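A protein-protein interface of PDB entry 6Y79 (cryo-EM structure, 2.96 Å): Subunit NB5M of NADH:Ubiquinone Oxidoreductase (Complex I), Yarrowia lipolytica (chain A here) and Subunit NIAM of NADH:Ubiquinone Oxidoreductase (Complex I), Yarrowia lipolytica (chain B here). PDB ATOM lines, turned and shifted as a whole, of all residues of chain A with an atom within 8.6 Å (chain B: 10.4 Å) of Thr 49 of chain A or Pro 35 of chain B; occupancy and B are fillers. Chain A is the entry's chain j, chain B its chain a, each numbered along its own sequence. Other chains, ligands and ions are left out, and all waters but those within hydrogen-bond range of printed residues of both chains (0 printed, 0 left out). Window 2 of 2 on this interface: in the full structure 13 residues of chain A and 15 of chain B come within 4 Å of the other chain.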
ATOM      1  N   TRP A  38      17.276 -20.716   2.499  1.00  0.00           N
ATOM      2  CA  TRP A  38      17.048 -19.497   1.749  1.00  0.00           C
ATOM      3  C   TRP A  38      18.181 -19.212   0.775  1.00  0.00           C
ATOM      4  O   TRP A  38      17.932 -18.679  -0.313  1.00  0.00           O
ATOM      5  CB  TRP A  38      16.869 -18.334   2.719  1.00  0.00           C
ATOM      6  CG  TRP A  38      16.498 -17.091   2.038  1.00  0.00           C
ATOM      7  CD1 TRP A  38      15.245 -16.673   1.746  1.00  0.00           C
ATOM      8  CD2 TRP A  38      17.384 -16.093   1.539  1.00  0.00           C
ATOM      9  NE1 TRP A  38      15.290 -15.473   1.096  1.00  0.00           N
ATOM     10  CE2 TRP A  38      16.596 -15.097   0.952  1.00  0.00           C
ATOM     11  CE3 TRP A  38      18.768 -15.949   1.526  1.00  0.00           C
ATOM     12  CZ2 TRP A  38      17.143 -13.970   0.364  1.00  0.00           C
ATOM     13  CZ3 TRP A  38      19.306 -14.835   0.940  1.00  0.00           C
ATOM     14  CH2 TRP A  38      18.498 -13.859   0.366  1.00  0.00           C
ATOM     15  N   TYR A  42      18.304 -19.537  -3.838  1.00  0.00           N
ATOM     16  CA  TYR A  42      18.262 -18.085  -3.985  1.00  0.00           C
ATOM     17  C   TYR A  42      17.777 -17.666  -5.361  1.00  0.00           C
ATOM     18  O   TYR A  42      17.272 -16.555  -5.534  1.00  0.00           O
ATOM     19  CB  TYR A  42      19.655 -17.513  -3.725  1.00  0.00           C
ATOM     20  CG  TYR A  42      19.790 -16.020  -3.889  1.00  0.00           C
ATOM     21  CD1 TYR A  42      19.396 -15.161  -2.885  1.00  0.00           C
ATOM     22  CD2 TYR A  42      20.321 -15.474  -5.050  1.00  0.00           C
ATOM     23  CE1 TYR A  42      19.519 -13.801  -3.030  1.00  0.00           C
ATOM     24  CE2 TYR A  42      20.443 -14.118  -5.207  1.00  0.00           C
ATOM     25  CZ  TYR A  42      20.043 -13.287  -4.193  1.00  0.00           C
ATOM     26  OH  TYR A  42      20.170 -11.930  -4.341  1.00  0.00           O
ATOM     27  N   ARG A  45      13.922 -16.815  -6.333  1.00  0.00           N
ATOM     28  CA  ARG A  45      13.436 -15.533  -5.856  1.00  0.00           C
ATOM     29  C   ARG A  45      14.313 -14.396  -6.349  1.00  0.00           C
ATOM     30  O   ARG A  45      14.132 -13.255  -5.918  1.00  0.00           O
ATOM     31  CB  ARG A  45      13.359 -15.532  -4.328  1.00  0.00           C
ATOM     32  CG  ARG A  45      14.696 -15.719  -3.655  1.00  0.00           C
ATOM     33  CD  ARG A  45      14.553 -15.766  -2.159  1.00  0.00           C
ATOM     34  NE  ARG A  45      13.845 -16.955  -1.710  1.00  0.00           N
ATOM     35  CZ  ARG A  45      14.445 -18.101  -1.419  1.00  0.00           C
ATOM     36  NH1 ARG A  45      15.760 -18.195  -1.530  1.00  0.00           N
ATOM     37  NH2 ARG A  45      13.740 -19.149  -1.012  1.00  0.00           N
ATOM     38  N   PHE A  46      15.247 -14.679  -7.246  1.00  0.00           N
ATOM     39  CA  PHE A  46      16.115 -13.654  -7.804  1.00  0.00           C
ATOM     40  C   PHE A  46      15.355 -12.786  -8.793  1.00  0.00           C
ATOM     41  O   PHE A  46      14.533 -13.278  -9.567  1.00  0.00           O
ATOM     42  CB  PHE A  46      17.303 -14.306  -8.496  1.00  0.00           C
ATOM     43  CG  PHE A  46      18.279 -13.338  -9.057  1.00  0.00           C
ATOM     44  CD1 PHE A  46      19.195 -12.727  -8.233  1.00  0.00           C
ATOM     45  CD2 PHE A  46      18.298 -13.049 -10.411  1.00  0.00           C
ATOM     46  CE1 PHE A  46      20.099 -11.838  -8.739  1.00  0.00           C
ATOM     47  CE2 PHE A  46      19.196 -12.153 -10.917  1.00  0.00           C
ATOM     48  CZ  PHE A  46      20.103 -11.566 -10.077  1.00  0.00           C
ATOM     49  N   LYS A  47      15.643 -11.485  -8.778  1.00  0.00           N
ATOM     50  CA  LYS A  47      14.987 -10.525  -9.653  1.00  0.00           C
ATOM     51  C   LYS A  47      16.000  -9.499 -10.132  1.00  0.00           C
ATOM     52  O   LYS A  47      16.999  -9.233  -9.465  1.00  0.00           O
ATOM     53  CB  LYS A  47      13.817  -9.810  -8.950  1.00  0.00           C
ATOM     54  CG  LYS A  47      12.589 -10.678  -8.746  1.00  0.00           C
ATOM     55  CD  LYS A  47      11.471  -9.956  -8.036  1.00  0.00           C
ATOM     56  CE  LYS A  47      10.327 -10.916  -7.757  1.00  0.00           C
ATOM     57  NZ  LYS A  47       9.126 -10.236  -7.198  1.00  0.00           N
ATOM     58  N   TYR A  48      15.719  -8.908 -11.289  1.00  0.00           N
ATOM     59  CA  TYR A  48      16.612  -7.927 -11.891  1.00  0.00           C
ATOM     60  C   TYR A  48      16.393  -6.544 -11.296  1.00  0.00           C
ATOM     61  O   TYR A  48      15.274  -6.021 -11.302  1.00  0.00           O
ATOM     62  CB  TYR A  48      16.406  -7.875 -13.398  1.00  0.00           C
ATOM     63  CG  TYR A  48      17.266  -8.865 -14.111  1.00  0.00           C
ATOM     64  CD1 TYR A  48      18.586  -8.579 -14.391  1.00  0.00           C
ATOM     65  CD2 TYR A  48      16.768 -10.103 -14.481  1.00  0.00           C
ATOM     66  CE1 TYR A  48      19.391  -9.495 -15.013  1.00  0.00           C
ATOM     67  CE2 TYR A  48      17.561 -11.024 -15.120  1.00  0.00           C
ATOM     68  CZ  TYR A  48      18.870 -10.714 -15.384  1.00  0.00           C
ATOM     69  OH  TYR A  48      19.665 -11.631 -16.022  1.00  0.00           O
ATOM     70  N   THR A  49      17.467  -5.957 -10.777  1.00  0.00           N
ATOM     71  CA  THR A  49      17.440  -4.621 -10.200  1.00  0.00           C
ATOM     72  C   THR A  49      18.554  -3.791 -10.815  1.00  0.00           C
ATOM     73  O   THR A  49      19.140  -4.189 -11.822  1.00  0.00           O
ATOM     74  CB  THR A  49      17.591  -4.668  -8.678  1.00  0.00           C
ATOM     75  OG1 THR A  49      18.759  -5.412  -8.319  1.00  0.00           O
ATOM     76  CG2 THR A  49      16.382  -5.293  -8.054  1.00  0.00           C
ATOM     77  N   ARG A  50      18.844  -2.630 -10.231  1.00  0.00           N
ATOM     78  CA  ARG A  50      19.958  -1.833 -10.727  1.00  0.00           C
ATOM     79  C   ARG A  50      21.298  -2.385 -10.257  1.00  0.00           C
ATOM     80  O   ARG A  50      22.267  -2.378 -11.024  1.00  0.00           O
ATOM     81  CB  ARG A  50      19.798  -0.380 -10.291  1.00  0.00           C
ATOM     82  CG  ARG A  50      20.857   0.544 -10.850  1.00  0.00           C
ATOM     83  CD  ARG A  50      20.668   1.969 -10.392  1.00  0.00           C
ATOM     84  NE  ARG A  50      21.762   2.813 -10.859  1.00  0.00           N
ATOM     85  CZ  ARG A  50      21.804   3.390 -12.055  1.00  0.00           C
ATOM     86  NH1 ARG A  50      22.847   4.137 -12.390  1.00  0.00           N
ATOM     87  NH2 ARG A  50      20.809   3.226 -12.914  1.00  0.00           N
ATOM     88  N   ALA A  51      21.375  -2.864  -9.011  1.00  0.00           N
ATOM     89  CA  ALA A  51      22.603  -3.483  -8.520  1.00  0.00           C
ATOM     90  C   ALA A  51      22.890  -4.779  -9.258  1.00  0.00           C
ATOM     91  O   ALA A  51      24.047  -5.072  -9.601  1.00  0.00           O
ATOM     92  CB  ALA A  51      22.493  -3.742  -7.021  1.00  0.00           C
ATOM     93  N   THR A  52      21.838  -5.553  -9.517  1.00  0.00           N
ATOM     94  CA  THR A  52      21.938  -6.738 -10.353  1.00  0.00           C
ATOM     95  C   THR A  52      22.424  -6.402 -11.756  1.00  0.00           C
ATOM     96  O   THR A  52      23.312  -7.074 -12.286  1.00  0.00           O
ATOM     97  CB  THR A  52      20.578  -7.417 -10.398  1.00  0.00           C
ATOM     98  OG1 THR A  52      20.311  -8.033  -9.133  1.00  0.00           O
ATOM     99  CG2 THR A  52      20.539  -8.434 -11.478  1.00  0.00           C
ATOM    100  N   GLY A  53      21.873  -5.351 -12.360  1.00  0.00           N
ATOM    101  CA  GLY A  53      22.286  -4.979 -13.701  1.00  0.00           C
ATOM    102  C   GLY A  53      23.714  -4.479 -13.768  1.00  0.00           C
ATOM    103  O   GLY A  53      24.436  -4.768 -14.728  1.00  0.00           O
ATOM    104  N   LYS A  54      24.136  -3.734 -12.743  1.00  0.00           N
ATOM    105  CA  LYS A  54      25.525  -3.313 -12.621  1.00  0.00           C
ATOM    106  C   LYS A  54      26.456  -4.513 -12.558  1.00  0.00           C
ATOM    107  O   LYS A  54      27.425  -4.593 -13.316  1.00  0.00           O
ATOM    108  CB  LYS A  54      25.690  -2.439 -11.382  1.00  0.00           C
ATOM    109  CG  LYS A  54      27.084  -1.887 -11.198  1.00  0.00           C
ATOM    110  CD  LYS A  54      27.152  -1.021  -9.960  1.00  0.00           C
ATOM    111  CE  LYS A  54      27.059  -1.866  -8.703  1.00  0.00           C
ATOM    112  NZ  LYS A  54      28.261  -2.731  -8.538  1.00  0.00           N
ATOM    113  N   SER A  55      26.134  -5.485 -11.697  1.00  0.00           N
ATOM    114  CA  SER A  55      26.967  -6.677 -11.555  1.00  0.00           C
ATOM    115  C   SER A  55      26.982  -7.518 -12.826  1.00  0.00           C
ATOM    116  O   SER A  55      28.036  -8.026 -13.228  1.00  0.00           O
ATOM    117  CB  SER A  55      26.472  -7.510 -10.378  1.00  0.00           C
ATOM    118  OG  SER A  55      26.573  -6.769  -9.181  1.00  0.00           O
ATOM    119  N   THR A  56      25.831  -7.641 -13.485  1.00  0.00           N
ATOM    120  CA  THR A  56      25.716  -8.478 -14.673  1.00  0.00           C
ATOM    121  C   THR A  56      26.502  -7.891 -15.837  1.00  0.00           C
ATOM    122  O   THR A  56      27.241  -8.606 -16.521  1.00  0.00           O
ATOM    123  CB  THR A  56      24.241  -8.649 -15.033  1.00  0.00           C
ATOM    124  OG1 THR A  56      23.590  -9.413 -14.011  1.00  0.00           O
ATOM    125  CG2 THR A  56      24.073  -9.351 -16.363  1.00  0.00           C
ATOM    126  N   ILE B  25      19.677  -3.900   5.884  1.00  0.00           N
ATOM    127  CA  ILE B  25      19.026  -2.609   5.993  1.00  0.00           C
ATOM    128  C   ILE B  25      20.059  -1.492   5.988  1.00  0.00           C
ATOM    129  O   ILE B  25      19.961  -0.565   5.186  1.00  0.00           O
ATOM    130  CB  ILE B  25      18.142  -2.530   7.253  1.00  0.00           C
ATOM    131  CG1 ILE B  25      17.049  -3.596   7.209  1.00  0.00           C
ATOM    132  CG2 ILE B  25      17.508  -1.165   7.373  1.00  0.00           C
ATOM    133  CD1 ILE B  25      16.169  -3.627   8.440  1.00  0.00           C
ATOM    134  N   ALA B  27      23.449  -1.372   5.393  1.00  0.00           N
ATOM    135  CA  ALA B  27      24.459  -1.281   4.350  1.00  0.00           C
ATOM    136  C   ALA B  27      23.815  -1.220   2.971  1.00  0.00           C
ATOM    137  O   ALA B  27      22.648  -1.569   2.787  1.00  0.00           O
ATOM    138  CB  ALA B  27      25.421  -2.459   4.428  1.00  0.00           C
ATOM    139  N   SER B  28      24.604  -0.763   1.996  1.00  0.00           N
ATOM    140  CA  SER B  28      24.074  -0.536   0.654  1.00  0.00           C
ATOM    141  C   SER B  28      23.815  -1.848  -0.079  1.00  0.00           C
ATOM    142  O   SER B  28      22.855  -1.956  -0.848  1.00  0.00           O
ATOM    143  CB  SER B  28      25.031   0.353  -0.137  1.00  0.00           C
ATOM    144  OG  SER B  28      26.275  -0.291  -0.342  1.00  0.00           O
ATOM    145  N   PHE B  29      24.651  -2.860   0.149  1.00  0.00           N
ATOM    146  CA  PHE B  29      24.409  -4.167  -0.454  1.00  0.00           C
ATOM    147  C   PHE B  29      23.283  -4.914   0.261  1.00  0.00           C
ATOM    148  O   PHE B  29      22.536  -5.680  -0.371  1.00  0.00           O
ATOM    149  CB  PHE B  29      25.710  -4.980  -0.468  1.00  0.00           C
ATOM    150  CG  PHE B  29      26.322  -5.195   0.892  1.00  0.00           C
ATOM    151  CD1 PHE B  29      27.244  -4.299   1.415  1.00  0.00           C
ATOM    152  CD2 PHE B  29      26.000  -6.317   1.634  1.00  0.00           C
ATOM    153  CE1 PHE B  29      27.801  -4.510   2.655  1.00  0.00           C
ATOM    154  CE2 PHE B  29      26.545  -6.525   2.874  1.00  0.00           C
ATOM    155  CZ  PHE B  29      27.449  -5.624   3.384  1.00  0.00           C
ATOM    156  N   ASP B  30      23.141  -4.690   1.572  1.00  0.00           N
ATOM    157  CA  ASP B  30      21.981  -5.184   2.302  1.00  0.00           C
ATOM    158  C   ASP B  30      20.702  -4.535   1.802  1.00  0.00           C
ATOM    159  O   ASP B  30      19.637  -5.162   1.815  1.00  0.00           O
ATOM    160  CB  ASP B  30      22.151  -4.916   3.795  1.00  0.00           C
ATOM    161  CG  ASP B  30      23.234  -5.760   4.420  1.00  0.00           C
ATOM    162  OD1 ASP B  30      23.393  -6.925   4.013  1.00  0.00           O
ATOM    163  OD2 ASP B  30      23.932  -5.258   5.321  1.00  0.00           O
ATOM    164  N   LYS B  31      20.789  -3.280   1.366  1.00  0.00           N
ATOM    165  CA  LYS B  31      19.674  -2.643   0.684  1.00  0.00           C
ATOM    166  C   LYS B  31      19.482  -3.222  -0.708  1.00  0.00           C
ATOM    167  O   LYS B  31      18.359  -3.262  -1.219  1.00  0.00           O
ATOM    168  CB  LYS B  31      19.918  -1.139   0.604  1.00  0.00           C
ATOM    169  CG  LYS B  31      18.671  -0.301   0.462  1.00  0.00           C
ATOM    170  CD  LYS B  31      19.002   1.162   0.659  1.00  0.00           C
ATOM    171  CE  LYS B  31      19.655   1.402   2.009  1.00  0.00           C
ATOM    172  NZ  LYS B  31      18.703   1.134   3.117  1.00  0.00           N
ATOM    173  N   ALA B  32      20.567  -3.657  -1.345  1.00  0.00           N
ATOM    174  CA  ALA B  32      20.477  -4.174  -2.702  1.00  0.00           C
ATOM    175  C   ALA B  32      19.805  -5.535  -2.761  1.00  0.00           C
ATOM    176  O   ALA B  32      19.233  -5.884  -3.798  1.00  0.00           O
ATOM    177  CB  ALA B  32      21.868  -4.263  -3.324  1.00  0.00           C
ATOM    178  N   GLU B  33      19.864  -6.317  -1.687  1.00  0.00           N
ATOM    179  CA  GLU B  33      19.211  -7.618  -1.733  1.00  0.00           C
ATOM    180  C   GLU B  33      17.818  -7.605  -1.111  1.00  0.00           C
ATOM    181  O   GLU B  33      17.219  -8.668  -0.936  1.00  0.00           O
ATOM    182  CB  GLU B  33      20.133  -8.649  -1.093  1.00  0.00           C
ATOM    183  CG  GLU B  33      21.389  -8.835  -1.955  1.00  0.00           C
ATOM    184  CD  GLU B  33      22.415  -9.768  -1.346  1.00  0.00           C
ATOM    185  OE1 GLU B  33      22.224 -10.164  -0.186  1.00  0.00           O
ATOM    186  OE2 GLU B  33      23.404 -10.092  -2.030  1.00  0.00           O
ATOM    187  N   GLU B  34      17.302  -6.421  -0.787  1.00  0.00           N
ATOM    188  CA  GLU B  34      15.927  -6.231  -0.314  1.00  0.00           C
ATOM    189  C   GLU B  34      14.822  -6.790  -1.216  1.00  0.00           C
ATOM    190  O   GLU B  34      13.909  -7.435  -0.678  1.00  0.00           O
ATOM    191  CB  GLU B  34      15.721  -4.732  -0.051  1.00  0.00           C
ATOM    192  CG  GLU B  34      14.394  -4.341   0.533  1.00  0.00           C
ATOM    193  CD  GLU B  34      14.340  -4.484   2.029  1.00  0.00           C
ATOM    194  OE1 GLU B  34      13.241  -4.296   2.586  1.00  0.00           O
ATOM    195  OE2 GLU B  34      15.388  -4.771   2.643  1.00  0.00           O
ATOM    196  N   PRO B  35      14.789  -6.575  -2.543  1.00  0.00           N
ATOM    197  CA  PRO B  35      13.647  -7.100  -3.308  1.00  0.00           C
ATOM    198  C   PRO B  35      13.731  -8.577  -3.652  1.00  0.00           C
ATOM    199  O   PRO B  35      12.763  -9.114  -4.203  1.00  0.00           O
ATOM    200  CB  PRO B  35      13.665  -6.253  -4.578  1.00  0.00           C
ATOM    201  CG  PRO B  35      15.049  -5.995  -4.777  1.00  0.00           C
ATOM    202  CD  PRO B  35      15.645  -5.770  -3.444  1.00  0.00           C
ATOM    203  N   MET B  36      14.844  -9.247  -3.357  1.00  0.00           N
ATOM    204  CA  MET B  36      14.946 -10.671  -3.652  1.00  0.00           C
ATOM    205  C   MET B  36      14.371 -11.526  -2.535  1.00  0.00           C
ATOM    206  O   MET B  36      13.863 -12.616  -2.802  1.00  0.00           O
ATOM    207  CB  MET B  36      16.398 -11.060  -3.925  1.00  0.00           C
ATOM    208  CG  MET B  36      16.819 -10.871  -5.370  1.00  0.00           C
ATOM    209  SD  MET B  36      17.101  -9.160  -5.821  1.00  0.00           S
ATOM    210  CE  MET B  36      18.782  -8.968  -5.257  1.00  0.00           C
ATOM    211  N   LEU B  37      14.425 -11.054  -1.294  1.00  0.00           N
ATOM    212  CA  LEU B  37      13.837 -11.808  -0.198  1.00  0.00           C
ATOM    213  C   LEU B  37      12.321 -11.742  -0.256  1.00  0.00           C
ATOM    214  O   LEU B  37      11.730 -10.693  -0.524  1.00  0.00           O
ATOM    215  CB  LEU B  37      14.334 -11.293   1.156  1.00  0.00           C
ATOM    216  CG  LEU B  37      14.191  -9.845   1.639  1.00  0.00           C
ATOM    217  CD1 LEU B  37      12.921  -9.612   2.431  1.00  0.00           C
ATOM    218  CD2 LEU B  37      15.378  -9.491   2.496  1.00  0.00           C
ATOM    219  N   GLY B  38      11.697 -12.880  -0.019  1.00  0.00           N
ATOM    220  CA  GLY B  38      10.281 -12.948   0.246  1.00  0.00           C
ATOM    221  C   GLY B  38      10.147 -14.076   1.235  1.00  0.00           C
ATOM    222  O   GLY B  38      10.901 -15.048   1.122  1.00  0.00           O
ATOM    223  N   ASP B  39       9.236 -13.942   2.205  1.00  0.00           N
ATOM    224  CA  ASP B  39       9.073 -14.868   3.333  1.00  0.00           C
ATOM    225  C   ASP B  39      10.387 -14.989   4.120  1.00  0.00           C
ATOM    226  O   ASP B  39      10.887 -16.075   4.420  1.00  0.00           O
ATOM    227  CB  ASP B  39       8.546 -16.226   2.841  1.00  0.00           C
ATOM    228  CG  ASP B  39       8.095 -17.139   3.962  1.00  0.00           C
ATOM    229  OD1 ASP B  39       7.772 -16.648   5.067  1.00  0.00           O
ATOM    230  OD2 ASP B  39       8.091 -18.366   3.731  1.00  0.00           O
ATOM    231  N   TYR B  40      10.973 -13.824   4.416  1.00  0.00           N
ATOM    232  CA  TYR B  40      12.240 -13.744   5.127  1.00  0.00           C
ATOM    233  C   TYR B  40      12.296 -12.441   5.923  1.00  0.00           C
ATOM    234  O   TYR B  40      12.018 -11.373   5.353  1.00  0.00           O
ATOM    235  CB  TYR B  40      13.426 -13.843   4.165  1.00  0.00           C
ATOM    236  CG  TYR B  40      14.729 -14.094   4.878  1.00  0.00           C
ATOM    237  CD1 TYR B  40      15.107 -15.378   5.254  1.00  0.00           C
ATOM    238  CD2 TYR B  40      15.561 -13.047   5.215  1.00  0.00           C
ATOM    239  CE1 TYR B  40      16.290 -15.603   5.932  1.00  0.00           C
ATOM    240  CE2 TYR B  40      16.712 -13.265   5.916  1.00  0.00           C
ATOM    241  CZ  TYR B  40      17.094 -14.541   6.242  1.00  0.00           C
ATOM    242  OH  TYR B  40      18.272 -14.740   6.913  1.00  0.00           O
ATOM    243  N   ASP B  42      14.009  -9.924   7.260  1.00  0.00           N
ATOM    244  CA  ASP B  42      14.671  -8.639   6.982  1.00  0.00           C
ATOM    245  C   ASP B  42      15.133  -7.945   8.272  1.00  0.00           C
ATOM    246  O   ASP B  42      14.597  -6.926   8.717  1.00  0.00           O
ATOM    247  CB  ASP B  42      13.784  -7.723   6.128  1.00  0.00           C
ATOM    248  CG  ASP B  42      14.530  -6.529   5.585  1.00  0.00           C
ATOM    249  OD1 ASP B  42      15.773  -6.471   5.698  1.00  0.00           O
ATOM    250  OD2 ASP B  42      13.864  -5.639   5.032  1.00  0.00           O
ATOM    251  N   VAL B  72      20.533 -11.545   5.976  1.00  0.00           N
ATOM    252  CA  VAL B  72      21.148 -11.886   4.706  1.00  0.00           C
ATOM    253  C   VAL B  72      22.520 -11.242   4.710  1.00  0.00           C
ATOM    254  O   VAL B  72      22.701 -10.162   5.292  1.00  0.00           O
ATOM    255  CB  VAL B  72      20.271 -11.423   3.531  1.00  0.00           C
ATOM    256  CG1 VAL B  72      20.834 -11.859   2.214  1.00  0.00           C
ATOM    257  CG2 VAL B  72      18.951 -12.006   3.643  1.00  0.00           C
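Printed residues of chain B that touch a printed residue of chain A: Ala 32, Pro 35, Met 36, Leu 37, Tyr 40 and Val 72. Printed residues of chain A that touch a printed residue of chain B: Trp 38, Tyr 42, Arg 45, Phe 46, Lys 47, Thr 49 and Ala 51. Hydrophobic or aromatic side chains of chain A within 4 Å of the printed part of chain B: Trp 38, Tyr 42 and Ala 51.
Thr 49 of chain A touches just one residue of chain B: Pro 35. Pro 35 of chain B touches one residue of chain A. Of chain B, only Ala 32 (3.8 Å) comes within 4 Å of Ala 51 of chain A. No residue of chain B comes within 4 Å of Thr 52 of chain A. Printed residues of chain A within 4 Å of Ala 32 of chain B: Ala 51 (3.8 Å). Of the printed residues of chain B, Arg 45 of chain A touches Met 36 (3.2 Å). Printed residues of chain A within 4 Å of Tyr 40 of chain B: Trp 38. Of the printed residues of chain A, Val 72 of chain B touches Trp 38. Of the printed residues of chain A, Leu 37 of chain B touches Trp 38 (3.96 Å). Tyr 48 of chain A touches none of the printed residues of chain B. The nearest residue of chain B that does not touch Thr 49 of chain A is Met 36 of chain B (4.5 Å). The nearest residue of chain A that does not touch Pro 35 of chain B is Lys 47 of chain A (4.1 Å).
O of Arg 45 of chain A lies close to O of Met 36 of chain B (3.2 Å). O of Lys 47 of chain A sits close to SD of Met 36 of chain B.
Among the printed residues, merely in contact across the chains: Tyr 42 of chain A with Met 36 of chain B (3.4 Å), Trp 38 of chain A with Val 72 of chain B (3.6 Å), Thr 49 of chain A with Pro 35 of chain B (3.6 Å), Trp 38 of chain A with Tyr 40 of chain B (3.7 Å), Phe 46 of chain A with Met 36 of chain B (3.8 Å), Ala 51 of chain A with Ala 32 of chain B (3.8 Å) and Trp 38 of chain A with Leu 37 of chain B (3.96 Å).
The backbone carbonyl oxygen of Trp 38 of chain A sits at hydrogen-bond distance from the guanidinium group of Arg 45 of chain A (2.5 Å). OG1 of Thr 52 of chain A sits at hydrogen-bond distance from OG1 of Thr 49 of chain A (3.2 Å). O of Ala 51 of chain A is in hydrogen-bond range of OG of Ser 55 of chain A (3.1 Å).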
